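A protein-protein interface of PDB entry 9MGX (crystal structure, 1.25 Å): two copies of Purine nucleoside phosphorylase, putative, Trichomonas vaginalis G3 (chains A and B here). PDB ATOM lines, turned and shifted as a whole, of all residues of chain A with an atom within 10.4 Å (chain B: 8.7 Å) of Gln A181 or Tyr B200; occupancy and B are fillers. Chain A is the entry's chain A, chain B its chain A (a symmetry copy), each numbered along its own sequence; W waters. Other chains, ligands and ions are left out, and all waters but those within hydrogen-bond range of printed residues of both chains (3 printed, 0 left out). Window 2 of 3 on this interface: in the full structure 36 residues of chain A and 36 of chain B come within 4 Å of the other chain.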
ATOM      1  N   THR A 102      15.634 -24.537  11.824  1.00  0.00           N
ATOM      2  CA  THR A 102      15.422 -24.463  13.261  1.00  0.00           C
ATOM      3  C   THR A 102      13.945 -24.270  13.562  1.00  0.00           C
ATOM      4  O   THR A 102      13.202 -23.690  12.768  1.00  0.00           O
ATOM      5  CB  THR A 102      16.239 -23.335  13.895  1.00  0.00           C
ATOM      6  OG1 THR A 102      16.198 -23.471  15.320  1.00  0.00           O
ATOM      7  CG2 THR A 102      15.681 -21.987  13.506  1.00  0.00           C
ATOM      8  N   VAL A 103      13.530 -24.795  14.715  1.00  0.00           N
ATOM      9  CA  VAL A 103      12.236 -24.492  15.318  1.00  0.00           C
ATOM     10  C   VAL A 103      12.380 -23.669  16.580  1.00  0.00           C
ATOM     11  O   VAL A 103      11.366 -23.287  17.169  1.00  0.00           O
ATOM     12  CB  VAL A 103      11.417 -25.761  15.637  1.00  0.00           C
ATOM     13  CG1 VAL A 103      11.140 -26.565  14.383  1.00  0.00           C
ATOM     14  CG2 VAL A 103      12.139 -26.593  16.703  1.00  0.00           C
ATOM     15  N   ASP A 104      13.601 -23.419  17.035  1.00  0.00           N
ATOM     16  CA  ASP A 104      13.791 -22.811  18.341  1.00  0.00           C
ATOM     17  C   ASP A 104      13.413 -21.337  18.262  1.00  0.00           C
ATOM     18  O   ASP A 104      13.837 -20.640  17.334  1.00  0.00           O
ATOM     19  CB  ASP A 104      15.247 -22.966  18.778  1.00  0.00           C
ATOM     20  CG  ASP A 104      15.480 -22.574  20.236  1.00  0.00           C
ATOM     21  OD1 ASP A 104      15.319 -21.389  20.585  1.00  0.00           O
ATOM     22  OD2 ASP A 104      15.829 -23.466  21.036  1.00  0.00           O
ATOM     23  N   PRO A 105      12.609 -20.829  19.193  1.00  0.00           N
ATOM     24  CA  PRO A 105      12.163 -19.433  19.076  1.00  0.00           C
ATOM     25  C   PRO A 105      13.290 -18.422  19.194  1.00  0.00           C
ATOM     26  O   PRO A 105      13.135 -17.285  18.726  1.00  0.00           O
ATOM     27  CB  PRO A 105      11.144 -19.291  20.213  1.00  0.00           C
ATOM     28  CG  PRO A 105      11.541 -20.341  21.207  1.00  0.00           C
ATOM     29  CD  PRO A 105      12.080 -21.486  20.401  1.00  0.00           C
ATOM     30  N   ASN A 106      14.416 -18.795  19.794  1.00  0.00           N
ATOM     31  CA  ASN A 106      15.529 -17.877  20.002  1.00  0.00           C
ATOM     32  C   ASN A 106      16.692 -18.145  19.062  1.00  0.00           C
ATOM     33  O   ASN A 106      17.782 -17.603  19.262  1.00  0.00           O
ATOM     34  CB  ASN A 106      15.977 -17.922  21.459  1.00  0.00           C
ATOM     35  CG  ASN A 106      14.918 -17.388  22.395  1.00  0.00           C
ATOM     36  OD1 ASN A 106      14.375 -16.299  22.183  1.00  0.00           O
ATOM     37  ND2 ASN A 106      14.587 -18.166  23.415  1.00  0.00           N
ATOM     38  N   LYS A 161      21.765 -29.100  20.859  1.00  0.00           N
ATOM     39  CA  LYS A 161      21.365 -30.336  20.200  1.00  0.00           C
ATOM     40  C   LYS A 161      20.855 -30.111  18.785  1.00  0.00           C
ATOM     41  O   LYS A 161      20.092 -29.180  18.528  1.00  0.00           O
ATOM     42  CB  LYS A 161      20.233 -31.007  20.984  1.00  0.00           C
ATOM     43  CG  LYS A 161      20.603 -31.482  22.391  1.00  0.00           C
ATOM     44  CD  LYS A 161      19.420 -32.154  23.079  1.00  0.00           C
ATOM     45  CE  LYS A 161      18.152 -31.302  23.190  1.00  0.00           C
ATOM     46  NZ  LYS A 161      18.369 -30.119  24.036  1.00  0.00           N
ATOM     47  N   GLY A 174       3.136 -32.714  15.597  1.00  0.00           N
ATOM     48  CA  GLY A 174       3.673 -32.611  16.927  1.00  0.00           C
ATOM     49  C   GLY A 174       5.181 -32.639  17.017  1.00  0.00           C
ATOM     50  O   GLY A 174       5.719 -32.349  18.085  1.00  0.00           O
ATOM     51  N   LEU A 175       5.888 -32.983  15.936  1.00  0.00           N
ATOM     52  CA  LEU A 175       7.348 -33.074  15.996  1.00  0.00           C
ATOM     53  C   LEU A 175       7.983 -31.718  16.290  1.00  0.00           C
ATOM     54  O   LEU A 175       8.830 -31.594  17.185  1.00  0.00           O
ATOM     55  CB  LEU A 175       7.893 -33.641  14.683  1.00  0.00           C
ATOM     56  CG  LEU A 175       9.423 -33.725  14.604  1.00  0.00           C
ATOM     57  CD1 LEU A 175       9.982 -34.732  15.598  1.00  0.00           C
ATOM     58  CD2 LEU A 175       9.871 -34.023  13.196  1.00  0.00           C
ATOM     59  N   ASN A 176       7.578 -30.679  15.557  1.00  0.00           N
ATOM     60  CA  ASN A 176       8.231 -29.386  15.731  1.00  0.00           C
ATOM     61  C   ASN A 176       8.017 -28.855  17.132  1.00  0.00           C
ATOM     62  O   ASN A 176       8.918 -28.252  17.718  1.00  0.00           O
ATOM     63  CB  ASN A 176       7.705 -28.384  14.717  1.00  0.00           C
ATOM     64  CG  ASN A 176       8.141 -28.710  13.309  1.00  0.00           C
ATOM     65  OD1 ASN A 176       9.175 -29.349  13.099  1.00  0.00           O
ATOM     66  ND2 ASN A 176       7.351 -28.277  12.331  1.00  0.00           N
ATOM     67  N   GLU A 177       6.826 -29.074  17.681  1.00  0.00           N
ATOM     68  CA  GLU A 177       6.535 -28.600  19.028  1.00  0.00           C
ATOM     69  C   GLU A 177       7.396 -29.310  20.065  1.00  0.00           C
ATOM     70  O   GLU A 177       7.871 -28.686  21.019  1.00  0.00           O
ATOM     71  CB  GLU A 177       5.047 -28.814  19.302  1.00  0.00           C
ATOM     72  CG  GLU A 177       4.106 -27.942  18.449  1.00  0.00           C
ATOM     73  CD  GLU A 177       3.805 -28.445  17.004  1.00  0.00           C
ATOM     74  OE1 GLU A 177       4.298 -29.497  16.512  1.00  0.00           O
ATOM     75  OE2 GLU A 177       3.012 -27.745  16.341  1.00  0.00           O
ATOM     76  N   ALA A 178       7.623 -30.609  19.899  1.00  0.00           N
ATOM     77  CA  ALA A 178       8.479 -31.331  20.839  1.00  0.00           C
ATOM     78  C   ALA A 178       9.932 -30.903  20.706  1.00  0.00           C
ATOM     79  O   ALA A 178      10.625 -30.713  21.713  1.00  0.00           O
ATOM     80  CB  ALA A 178       8.340 -32.831  20.601  1.00  0.00           C
ATOM     81  N   LEU A 179      10.413 -30.745  19.477  1.00  0.00           N
ATOM     82  CA  LEU A 179      11.776 -30.259  19.276  1.00  0.00           C
ATOM     83  C   LEU A 179      11.981 -28.898  19.931  1.00  0.00           C
ATOM     84  O   LEU A 179      13.026 -28.643  20.539  1.00  0.00           O
ATOM     85  CB  LEU A 179      12.107 -30.208  17.783  1.00  0.00           C
ATOM     86  CG  LEU A 179      12.172 -31.542  17.045  1.00  0.00           C
ATOM     87  CD1 LEU A 179      12.307 -31.311  15.548  1.00  0.00           C
ATOM     88  CD2 LEU A 179      13.345 -32.372  17.559  1.00  0.00           C
ATOM     89  N   ALA A 180      10.990 -28.010  19.819  1.00  0.00           N
ATOM     90  CA  ALA A 180      11.097 -26.690  20.430  1.00  0.00           C
ATOM     91  C   ALA A 180      11.038 -26.772  21.950  1.00  0.00           C
ATOM     92  O   ALA A 180      11.785 -26.067  22.642  1.00  0.00           O
ATOM     93  CB  ALA A 180       9.980 -25.781  19.913  1.00  0.00           C
ATOM     94  N   GLN A 181      10.162 -27.630  22.487  1.00  0.00           N
ATOM     95  CA  GLN A 181      10.012 -27.754  23.932  1.00  0.00           C
ATOM     96  C   GLN A 181      11.332 -28.124  24.587  1.00  0.00           C
ATOM     97  O   GLN A 181      11.623 -27.703  25.707  1.00  0.00           O
ATOM     98  CB  GLN A 181       8.967 -28.825  24.247  1.00  0.00           C
ATOM     99  CG  GLN A 181       8.739 -29.066  25.740  1.00  0.00           C
ATOM    100  CD  GLN A 181       8.044 -27.917  26.396  1.00  0.00           C
ATOM    101  OE1 GLN A 181       6.853 -27.712  26.192  1.00  0.00           O
ATOM    102  NE2 GLN A 181       8.776 -27.166  27.225  1.00  0.00           N
ATOM    103  N   TYR A 182      12.119 -28.958  23.932  1.00  0.00           N
ATOM    104  CA  TYR A 182      13.367 -29.452  24.499  1.00  0.00           C
ATOM    105  C   TYR A 182      14.583 -28.735  23.932  1.00  0.00           C
ATOM    106  O   TYR A 182      15.710 -29.191  24.145  1.00  0.00           O
ATOM    107  CB  TYR A 182      13.443 -30.980  24.361  1.00  0.00           C
ATOM    108  CG  TYR A 182      12.395 -31.640  25.223  1.00  0.00           C
ATOM    109  CD1 TYR A 182      12.620 -31.836  26.573  1.00  0.00           C
ATOM    110  CD2 TYR A 182      11.173 -32.034  24.708  1.00  0.00           C
ATOM    111  CE1 TYR A 182      11.662 -32.404  27.383  1.00  0.00           C
ATOM    112  CE2 TYR A 182      10.197 -32.601  25.527  1.00  0.00           C
ATOM    113  CZ  TYR A 182      10.454 -32.790  26.858  1.00  0.00           C
ATOM    114  OH  TYR A 182       9.506 -33.338  27.689  1.00  0.00           O
ATOM    115  N   HIS A 183      14.375 -27.641  23.207  1.00  0.00           N
ATOM    116  CA  HIS A 183      15.458 -26.742  22.804  1.00  0.00           C
ATOM    117  C   HIS A 183      16.472 -27.415  21.885  1.00  0.00           C
ATOM    118  O   HIS A 183      17.673 -27.189  21.989  1.00  0.00           O
ATOM    119  CB  HIS A 183      16.123 -26.075  24.008  1.00  0.00           C
ATOM    120  CG  HIS A 183      15.204 -25.166  24.748  1.00  0.00           C
ATOM    121  ND1 HIS A 183      15.007 -23.855  24.381  1.00  0.00           N
ATOM    122  CD2 HIS A 183      14.399 -25.382  25.809  1.00  0.00           C
ATOM    123  CE1 HIS A 183      14.142 -23.294  25.206  1.00  0.00           C
ATOM    124  NE2 HIS A 183      13.745 -24.207  26.072  1.00  0.00           N
ATOM    125  N   PHE A 184      15.977 -28.200  20.933  1.00  0.00           N
ATOM    126  CA  PHE A 184      16.787 -28.596  19.788  1.00  0.00           C
ATOM    127  C   PHE A 184      17.001 -27.370  18.916  1.00  0.00           C
ATOM    128  O   PHE A 184      16.039 -26.691  18.556  1.00  0.00           O
ATOM    129  CB  PHE A 184      16.089 -29.703  18.997  1.00  0.00           C
ATOM    130  CG  PHE A 184      16.143 -31.056  19.668  1.00  0.00           C
ATOM    131  CD1 PHE A 184      15.246 -31.406  20.679  1.00  0.00           C
ATOM    132  CD2 PHE A 184      17.106 -31.979  19.306  1.00  0.00           C
ATOM    133  CE1 PHE A 184      15.319 -32.646  21.282  1.00  0.00           C
ATOM    134  CE2 PHE A 184      17.181 -33.204  19.906  1.00  0.00           C
ATOM    135  CZ  PHE A 184      16.278 -33.538  20.886  1.00  0.00           C
ATOM    136  N   ILE A 185      18.259 -27.069  18.588  1.00  0.00           N
ATOM    137  CA  ILE A 185      18.576 -25.835  17.873  1.00  0.00           C
ATOM    138  C   ILE A 185      18.675 -26.016  16.367  1.00  0.00           C
ATOM    139  O   ILE A 185      18.549 -25.022  15.640  1.00  0.00           O
ATOM    140  CB  ILE A 185      19.837 -25.131  18.420  1.00  0.00           C
ATOM    141  CG1 ILE A 185      21.093 -25.974  18.202  1.00  0.00           C
ATOM    142  CG2 ILE A 185      19.650 -24.792  19.891  1.00  0.00           C
ATOM    143  CD1 ILE A 185      22.381 -25.243  18.568  1.00  0.00           C
ATOM    144  N   ILE A 216       9.213 -22.658  11.730  1.00  0.00           N
ATOM    145  CA  ILE A 216       7.965 -22.146  12.290  1.00  0.00           C
ATOM    146  C   ILE A 216       7.539 -20.864  11.583  1.00  0.00           C
ATOM    147  O   ILE A 216       6.418 -20.775  11.065  1.00  0.00           O
ATOM    148  CB  ILE A 216       8.081 -21.916  13.809  1.00  0.00           C
ATOM    149  CG1 ILE A 216       8.570 -23.182  14.524  1.00  0.00           C
ATOM    150  CG2 ILE A 216       6.745 -21.466  14.386  1.00  0.00           C
ATOM    151  CD1 ILE A 216       7.681 -24.393  14.322  1.00  0.00           C
ATOM    152  N   GLU B  83      12.673 -32.447  38.495  1.00  0.00           N
ATOM    153  CA  GLU B  83      11.515 -31.730  37.985  1.00  0.00           C
ATOM    154  C   GLU B  83      11.061 -30.685  38.994  1.00  0.00           C
ATOM    155  O   GLU B  83      10.788 -29.532  38.658  1.00  0.00           O
ATOM    156  CB  GLU B  83      10.379 -32.714  37.696  1.00  0.00           C
ATOM    157  CG  GLU B  83       9.138 -32.076  37.077  1.00  0.00           C
ATOM    158  CD  GLU B  83       9.073 -32.195  35.567  1.00  0.00           C
ATOM    159  OE1 GLU B  83       9.830 -32.986  34.967  1.00  0.00           O
ATOM    160  OE2 GLU B  83       8.230 -31.489  34.975  1.00  0.00           O
ATOM    161  N   TYR B  86      13.641 -27.660  39.289  1.00  0.00           N
ATOM    162  CA  TYR B  86      13.564 -26.702  38.185  1.00  0.00           C
ATOM    163  C   TYR B  86      12.223 -25.969  38.164  1.00  0.00           C
ATOM    164  O   TYR B  86      12.171 -24.773  37.882  1.00  0.00           O
ATOM    165  CB  TYR B  86      13.793 -27.394  36.835  1.00  0.00           C
ATOM    166  CG  TYR B  86      15.198 -27.874  36.564  1.00  0.00           C
ATOM    167  CD1 TYR B  86      16.266 -26.995  36.546  1.00  0.00           C
ATOM    168  CD2 TYR B  86      15.462 -29.204  36.309  1.00  0.00           C
ATOM    169  CE1 TYR B  86      17.546 -27.437  36.265  1.00  0.00           C
ATOM    170  CE2 TYR B  86      16.728 -29.646  36.022  1.00  0.00           C
ATOM    171  CZ  TYR B  86      17.775 -28.752  35.992  1.00  0.00           C
ATOM    172  OH  TYR B  86      19.030 -29.238  35.715  1.00  0.00           O
ATOM    173  N   ASN B  87      11.126 -26.672  38.438  1.00  0.00           N
ATOM    174  CA  ASN B  87       9.798 -26.089  38.260  1.00  0.00           C
ATOM    175  C   ASN B  87       9.372 -25.247  39.461  1.00  0.00           C
ATOM    176  O   ASN B  87       9.058 -24.068  39.317  1.00  0.00           O
ATOM    177  CB  ASN B  87       8.804 -27.218  37.998  1.00  0.00           C
ATOM    178  CG  ASN B  87       7.410 -26.726  37.704  1.00  0.00           C
ATOM    179  OD1 ASN B  87       7.206 -25.784  36.931  1.00  0.00           O
ATOM    180  ND2 ASN B  87       6.427 -27.388  38.304  1.00  0.00           N
ATOM    181  N   ARG B 128       9.233 -38.528  25.440  1.00  0.00           N
ATOM    182  CA  ARG B 128       9.253 -37.087  25.280  1.00  0.00           C
ATOM    183  C   ARG B 128       9.374 -36.651  23.828  1.00  0.00           C
ATOM    184  O   ARG B 128       9.063 -35.497  23.518  1.00  0.00           O
ATOM    185  CB  ARG B 128      10.448 -36.509  26.055  1.00  0.00           C
ATOM    186  CG  ARG B 128      10.333 -36.659  27.553  1.00  0.00           C
ATOM    187  CD  ARG B 128      11.616 -36.219  28.283  1.00  0.00           C
ATOM    188  NE  ARG B 128      11.368 -36.057  29.711  1.00  0.00           N
ATOM    189  CZ  ARG B 128      11.846 -36.783  30.705  1.00  0.00           C
ATOM    190  NH1 ARG B 128      12.746 -37.734  30.512  1.00  0.00           N
ATOM    191  NH2 ARG B 128      11.414 -36.536  31.944  1.00  0.00           N
ATOM    192  N   LEU B 129       9.830 -37.519  22.932  1.00  0.00           N
ATOM    193  CA  LEU B 129      10.155 -37.112  21.569  1.00  0.00           C
ATOM    194  C   LEU B 129       9.492 -38.031  20.549  1.00  0.00           C
ATOM    195  O   LEU B 129      10.106 -38.487  19.582  1.00  0.00           O
ATOM    196  CB  LEU B 129      11.670 -36.994  21.364  1.00  0.00           C
ATOM    197  CG  LEU B 129      12.075 -36.141  20.161  1.00  0.00           C
ATOM    198  CD1 LEU B 129      11.611 -34.713  20.314  1.00  0.00           C
ATOM    199  CD2 LEU B 129      13.578 -36.174  19.964  1.00  0.00           C
ATOM    200  N   PHE B 134      16.211 -39.266  21.514  1.00  0.00           N
ATOM    201  CA  PHE B 134      16.433 -37.962  22.150  1.00  0.00           C
ATOM    202  C   PHE B 134      17.686 -38.087  22.996  1.00  0.00           C
ATOM    203  O   PHE B 134      17.649 -38.745  24.048  1.00  0.00           O
ATOM    204  CB  PHE B 134      15.208 -37.708  23.029  1.00  0.00           C
ATOM    205  CG  PHE B 134      15.194 -36.407  23.811  1.00  0.00           C
ATOM    206  CD1 PHE B 134      16.293 -35.580  23.959  1.00  0.00           C
ATOM    207  CD2 PHE B 134      14.022 -36.035  24.433  1.00  0.00           C
ATOM    208  CE1 PHE B 134      16.208 -34.424  24.714  1.00  0.00           C
ATOM    209  CE2 PHE B 134      13.951 -34.885  25.184  1.00  0.00           C
ATOM    210  CZ  PHE B 134      15.051 -34.088  25.334  1.00  0.00           C
ATOM    211  N   LEU B 194      18.134 -36.781  33.946  1.00  0.00           N
ATOM    212  CA  LEU B 194      18.285 -35.392  34.372  1.00  0.00           C
ATOM    213  C   LEU B 194      18.325 -34.434  33.189  1.00  0.00           C
ATOM    214  O   LEU B 194      17.645 -33.401  33.192  1.00  0.00           O
ATOM    215  CB  LEU B 194      19.567 -35.266  35.184  1.00  0.00           C
ATOM    216  CG  LEU B 194      19.979 -33.860  35.615  1.00  0.00           C
ATOM    217  CD1 LEU B 194      18.935 -33.223  36.503  1.00  0.00           C
ATOM    218  CD2 LEU B 194      21.316 -33.882  36.329  1.00  0.00           C
ATOM    219  N   PHE B 195      19.137 -34.743  32.172  1.00  0.00           N
ATOM    220  CA  PHE B 195      19.409 -33.765  31.126  1.00  0.00           C
ATOM    221  C   PHE B 195      18.149 -33.346  30.375  1.00  0.00           C
ATOM    222  O   PHE B 195      17.998 -32.141  30.099  1.00  0.00           O
ATOM    223  CB  PHE B 195      20.501 -34.276  30.168  1.00  0.00           C
ATOM    224  CG  PHE B 195      21.815 -34.611  30.842  1.00  0.00           C
ATOM    225  CD1 PHE B 195      22.243 -33.941  31.988  1.00  0.00           C
ATOM    226  CD2 PHE B 195      22.632 -35.592  30.337  1.00  0.00           C
ATOM    227  CE1 PHE B 195      23.457 -34.248  32.586  1.00  0.00           C
ATOM    228  CE2 PHE B 195      23.837 -35.913  30.936  1.00  0.00           C
ATOM    229  CZ  PHE B 195      24.262 -35.215  32.044  1.00  0.00           C
ATOM    230  N   PRO B 196      17.217 -34.243  30.028  1.00  0.00           N
ATOM    231  CA  PRO B 196      16.028 -33.788  29.293  1.00  0.00           C
ATOM    232  C   PRO B 196      15.092 -32.937  30.123  1.00  0.00           C
ATOM    233  O   PRO B 196      14.365 -32.101  29.567  1.00  0.00           O
ATOM    234  CB  PRO B 196      15.376 -35.099  28.852  1.00  0.00           C
ATOM    235  CG  PRO B 196      16.532 -36.048  28.771  1.00  0.00           C
ATOM    236  CD  PRO B 196      17.315 -35.709  29.997  1.00  0.00           C
ATOM    237  N   ILE B 197      15.078 -33.123  31.442  1.00  0.00           N
ATOM    238  CA  ILE B 197      14.263 -32.274  32.307  1.00  0.00           C
ATOM    239  C   ILE B 197      14.821 -30.862  32.327  1.00  0.00           C
ATOM    240  O   ILE B 197      14.067 -29.883  32.245  1.00  0.00           O
ATOM    241  CB  ILE B 197      14.148 -32.887  33.718  1.00  0.00           C
ATOM    242  CG1 ILE B 197      13.428 -34.237  33.643  1.00  0.00           C
ATOM    243  CG2 ILE B 197      13.442 -31.954  34.681  1.00  0.00           C
ATOM    244  CD1 ILE B 197      13.373 -34.989  34.962  1.00  0.00           C
ATOM    245  N   ALA B 198      16.141 -30.728  32.454  1.00  0.00           N
ATOM    246  CA  ALA B 198      16.746 -29.407  32.325  1.00  0.00           C
ATOM    247  C   ALA B 198      16.331 -28.759  31.011  1.00  0.00           C
ATOM    248  O   ALA B 198      15.960 -27.587  30.983  1.00  0.00           O
ATOM    249  CB  ALA B 198      18.263 -29.514  32.420  1.00  0.00           C
ATOM    250  N   ASP B 199      16.378 -29.518  29.903  1.00  0.00           N
ATOM    251  CA  ASP B 199      15.959 -28.979  28.607  1.00  0.00           C
ATOM    252  C   ASP B 199      14.528 -28.456  28.653  1.00  0.00           C
ATOM    253  O   ASP B 199      14.238 -27.367  28.157  1.00  0.00           O
ATOM    254  CB  ASP B 199      16.048 -30.049  27.517  1.00  0.00           C
ATOM    255  CG  ASP B 199      17.452 -30.434  27.140  1.00  0.00           C
ATOM    256  OD1 ASP B 199      18.409 -29.686  27.440  1.00  0.00           O
ATOM    257  OD2 ASP B 199      17.587 -31.513  26.517  1.00  0.00           O
ATOM    258  N   TYR B 200      13.607 -29.240  29.222  1.00  0.00           N
ATOM    259  CA  TYR B 200      12.202 -28.848  29.252  1.00  0.00           C
ATOM    260  C   TYR B 200      12.041 -27.469  29.868  1.00  0.00           C
ATOM    261  O   TYR B 200      11.198 -26.680  29.432  1.00  0.00           O
ATOM    262  CB  TYR B 200      11.409 -29.880  30.067  1.00  0.00           C
ATOM    263  CG  TYR B 200       9.918 -29.622  30.126  1.00  0.00           C
ATOM    264  CD1 TYR B 200       9.374 -28.822  31.132  1.00  0.00           C
ATOM    265  CD2 TYR B 200       9.052 -30.158  29.182  1.00  0.00           C
ATOM    266  CE1 TYR B 200       8.022 -28.575  31.190  1.00  0.00           C
ATOM    267  CE2 TYR B 200       7.703 -29.907  29.231  1.00  0.00           C
ATOM    268  CZ  TYR B 200       7.195 -29.121  30.234  1.00  0.00           C
ATOM    269  OH  TYR B 200       5.845 -28.881  30.282  1.00  0.00           O
ATOM    270  N   TYR B 201      12.807 -27.184  30.923  1.00  0.00           N
ATOM    271  CA  TYR B 201      12.715 -25.935  31.674  1.00  0.00           C
ATOM    272  C   TYR B 201      13.664 -24.861  31.169  1.00  0.00           C
ATOM    273  O   TYR B 201      13.748 -23.791  31.784  1.00  0.00           O
ATOM    274  CB  TYR B 201      12.913 -26.206  33.179  1.00  0.00           C
ATOM    275  CG  TYR B 201      11.717 -26.935  33.736  1.00  0.00           C
ATOM    276  CD1 TYR B 201      10.536 -26.261  33.958  1.00  0.00           C
ATOM    277  CD2 TYR B 201      11.748 -28.295  33.980  1.00  0.00           C
ATOM    278  CE1 TYR B 201       9.417 -26.914  34.406  1.00  0.00           C
ATOM    279  CE2 TYR B 201      10.636 -28.962  34.450  1.00  0.00           C
ATOM    280  CZ  TYR B 201       9.473 -28.266  34.645  1.00  0.00           C
ATOM    281  OH  TYR B 201       8.319 -28.897  35.087  1.00  0.00           O
ATOM    282  N   GLY B 202      14.354 -25.091  30.052  1.00  0.00           N
ATOM    283  CA  GLY B 202      15.288 -24.087  29.553  1.00  0.00           C
ATOM    284  C   GLY B 202      16.449 -23.862  30.488  1.00  0.00           C
ATOM    285  O   GLY B 202      17.005 -22.757  30.532  1.00  0.00           O
ATOM    286  N   ALA B 203      16.817 -24.877  31.247  1.00  0.00           N
ATOM    287  CA  ALA B 203      17.812 -24.798  32.301  1.00  0.00           C
ATOM    288  C   ALA B 203      19.014 -25.672  31.935  1.00  0.00           C
ATOM    289  O   ALA B 203      19.105 -26.187  30.823  1.00  0.00           O
ATOM    290  CB  ALA B 203      17.170 -25.186  33.628  1.00  0.00           C
ATOM    291  N   ARG B 204      19.952 -25.813  32.869  1.00  0.00           N
ATOM    292  CA  ARG B 204      21.231 -26.447  32.603  1.00  0.00           C
ATOM    293  C   ARG B 204      21.482 -27.599  33.561  1.00  0.00           C
ATOM    294  O   ARG B 204      21.096 -27.557  34.733  1.00  0.00           O
ATOM    295  CB  ARG B 204      22.371 -25.433  32.734  1.00  0.00           C
ATOM    296  CG  ARG B 204      22.247 -24.283  31.762  1.00  0.00           C
ATOM    297  CD  ARG B 204      23.453 -23.390  31.830  1.00  0.00           C
ATOM    298  NE  ARG B 204      23.685 -22.923  33.189  1.00  0.00           N
ATOM    299  CZ  ARG B 204      24.602 -22.036  33.524  1.00  0.00           C
ATOM    300  NH1 ARG B 204      25.397 -21.491  32.619  1.00  0.00           N
ATOM    301  NH2 ARG B 204      24.719 -21.682  34.802  1.00  0.00           N
HETATM  302  O   HOH W   1       9.673 -33.915  30.433  1.00  0.00           O
HETATM  303  O   HOH W   2      11.436 -24.958  27.412  1.00  0.00           O
HETATM  304  O   HOH W   3      20.676 -30.652  26.397  1.00  0.00           O
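Asn A176 touches none of the printed residues of chain B. No residue of chain B comes within 4 Å of Ala A180. Printed residues of chain B within 4 Å of Tyr A182: Arg B128, Phe B134, Pro B196, Asp B199 and Tyr B200. Of the printed residues of chain B, His A183 touches Asp B199 (3.1 Å) and Gly B202 (3.8 Å). Of the printed residues of chain B, Phe A184 touches Leu B129 and Phe B134. Of the printed residues of chain A, Arg B128 touches Tyr A182. Of the printed residues of chain A, Phe B134 touches Lys A161 (3.98 Å), Tyr A182 (3.5 Å) and Phe A184 (3.7 Å). No residue of chain A comes within 4 Å of Ala B198. Of chain A, only Gln A181 (3.3 Å) and Tyr A182 (3.5 Å) come within 4 Å of Tyr B200. Of the printed residues of chain A, Gly B202 touches His A183. The nearest residue of chain B that does not touch Gln A181 is Tyr B201 (5.4 Å). The nearest printed residue of chain B that does not touch His A183 is Tyr B200 (4.9 Å).
OD2 of Asp A104 sits at hydrogen-bond distance from ND1 of His A183. NZ of Lys A161 lies within hydrogen-bond range of O of Tyr A182 (2.8 Å). The backbone carbonyl oxygen (O) of Lys A161 lies within hydrogen-bond range of the backbone NH (N) of Ile A185 (2.8 Å). O of Leu A179 is in hydrogen-bond range of N of Phe A184 (3.0 Å).
Water W2 lies within hydrogen-bond range of O of Tyr B200 (2.7 Å), NE2 of His A183 (2.8 Å) and O of Gln A181 (3.2 Å). Water W3 lies within hydrogen-bond range of OD1 of Asp B199 (2.7 Å) and NZ of Lys A161 (3.3 Å). Water W1 bridges OH of Tyr A182 (2.8 Å) and NE of Arg B128 (2.8 Å).
No position is printed for both chains.
The side-chain carboxylate (OD2) of Asp B199 lies within salt-bridge range of the side-chain amino group (NZ) of Lys A161 (3.0 Å). NE2 of Gln A181 lies within hydrogen-bond range of O of Tyr B200, 3.3 Å away.
Of the 17 printed residues of chain B, 7 touch a printed residue of chain A. Printed residues of chain B that touch a printed residue of chain A: Arg B128, Leu B129, Phe B134, Pro B196, Asp B199, Tyr B200 and Gly B202. Of the 19 printed residues of chain A, 6 touch a printed residue of chain B. Printed residues of chain A that touch a printed residue of chain B: Lys A161, Ala A178, Gln A181, Tyr A182, His A183 and Phe A184. Hydrophobic or aromatic side chains of chain A that line the printed part of chain B: Ala A178, Tyr A182, His A183 and Phe A184. Among the printed residues, 14 pairs touch across the chains.
Among the printed residues, pairs that only touch across the chains: Lys A161 with Phe B134 (3.98 Å), Ala A178 with Leu B129 (3.8 Å), Gln A181 with Asp B199 (3.6 Å), Tyr A182 with Arg B128 (3.4 Å), Tyr A182 with Phe B134 (3.5 Å), Tyr A182 with Pro B196 (3.5 Å), Tyr A182 with Asp B199 (3.5 Å), Tyr A182 with Tyr B200 (3.5 Å), His A183 with Asp B199 (3.1 Å), His A183 with Gly B202 (3.8 Å), Phe A184 with Leu B129 (3.9 Å) and Phe A184 with Phe B134 (3.7 Å).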
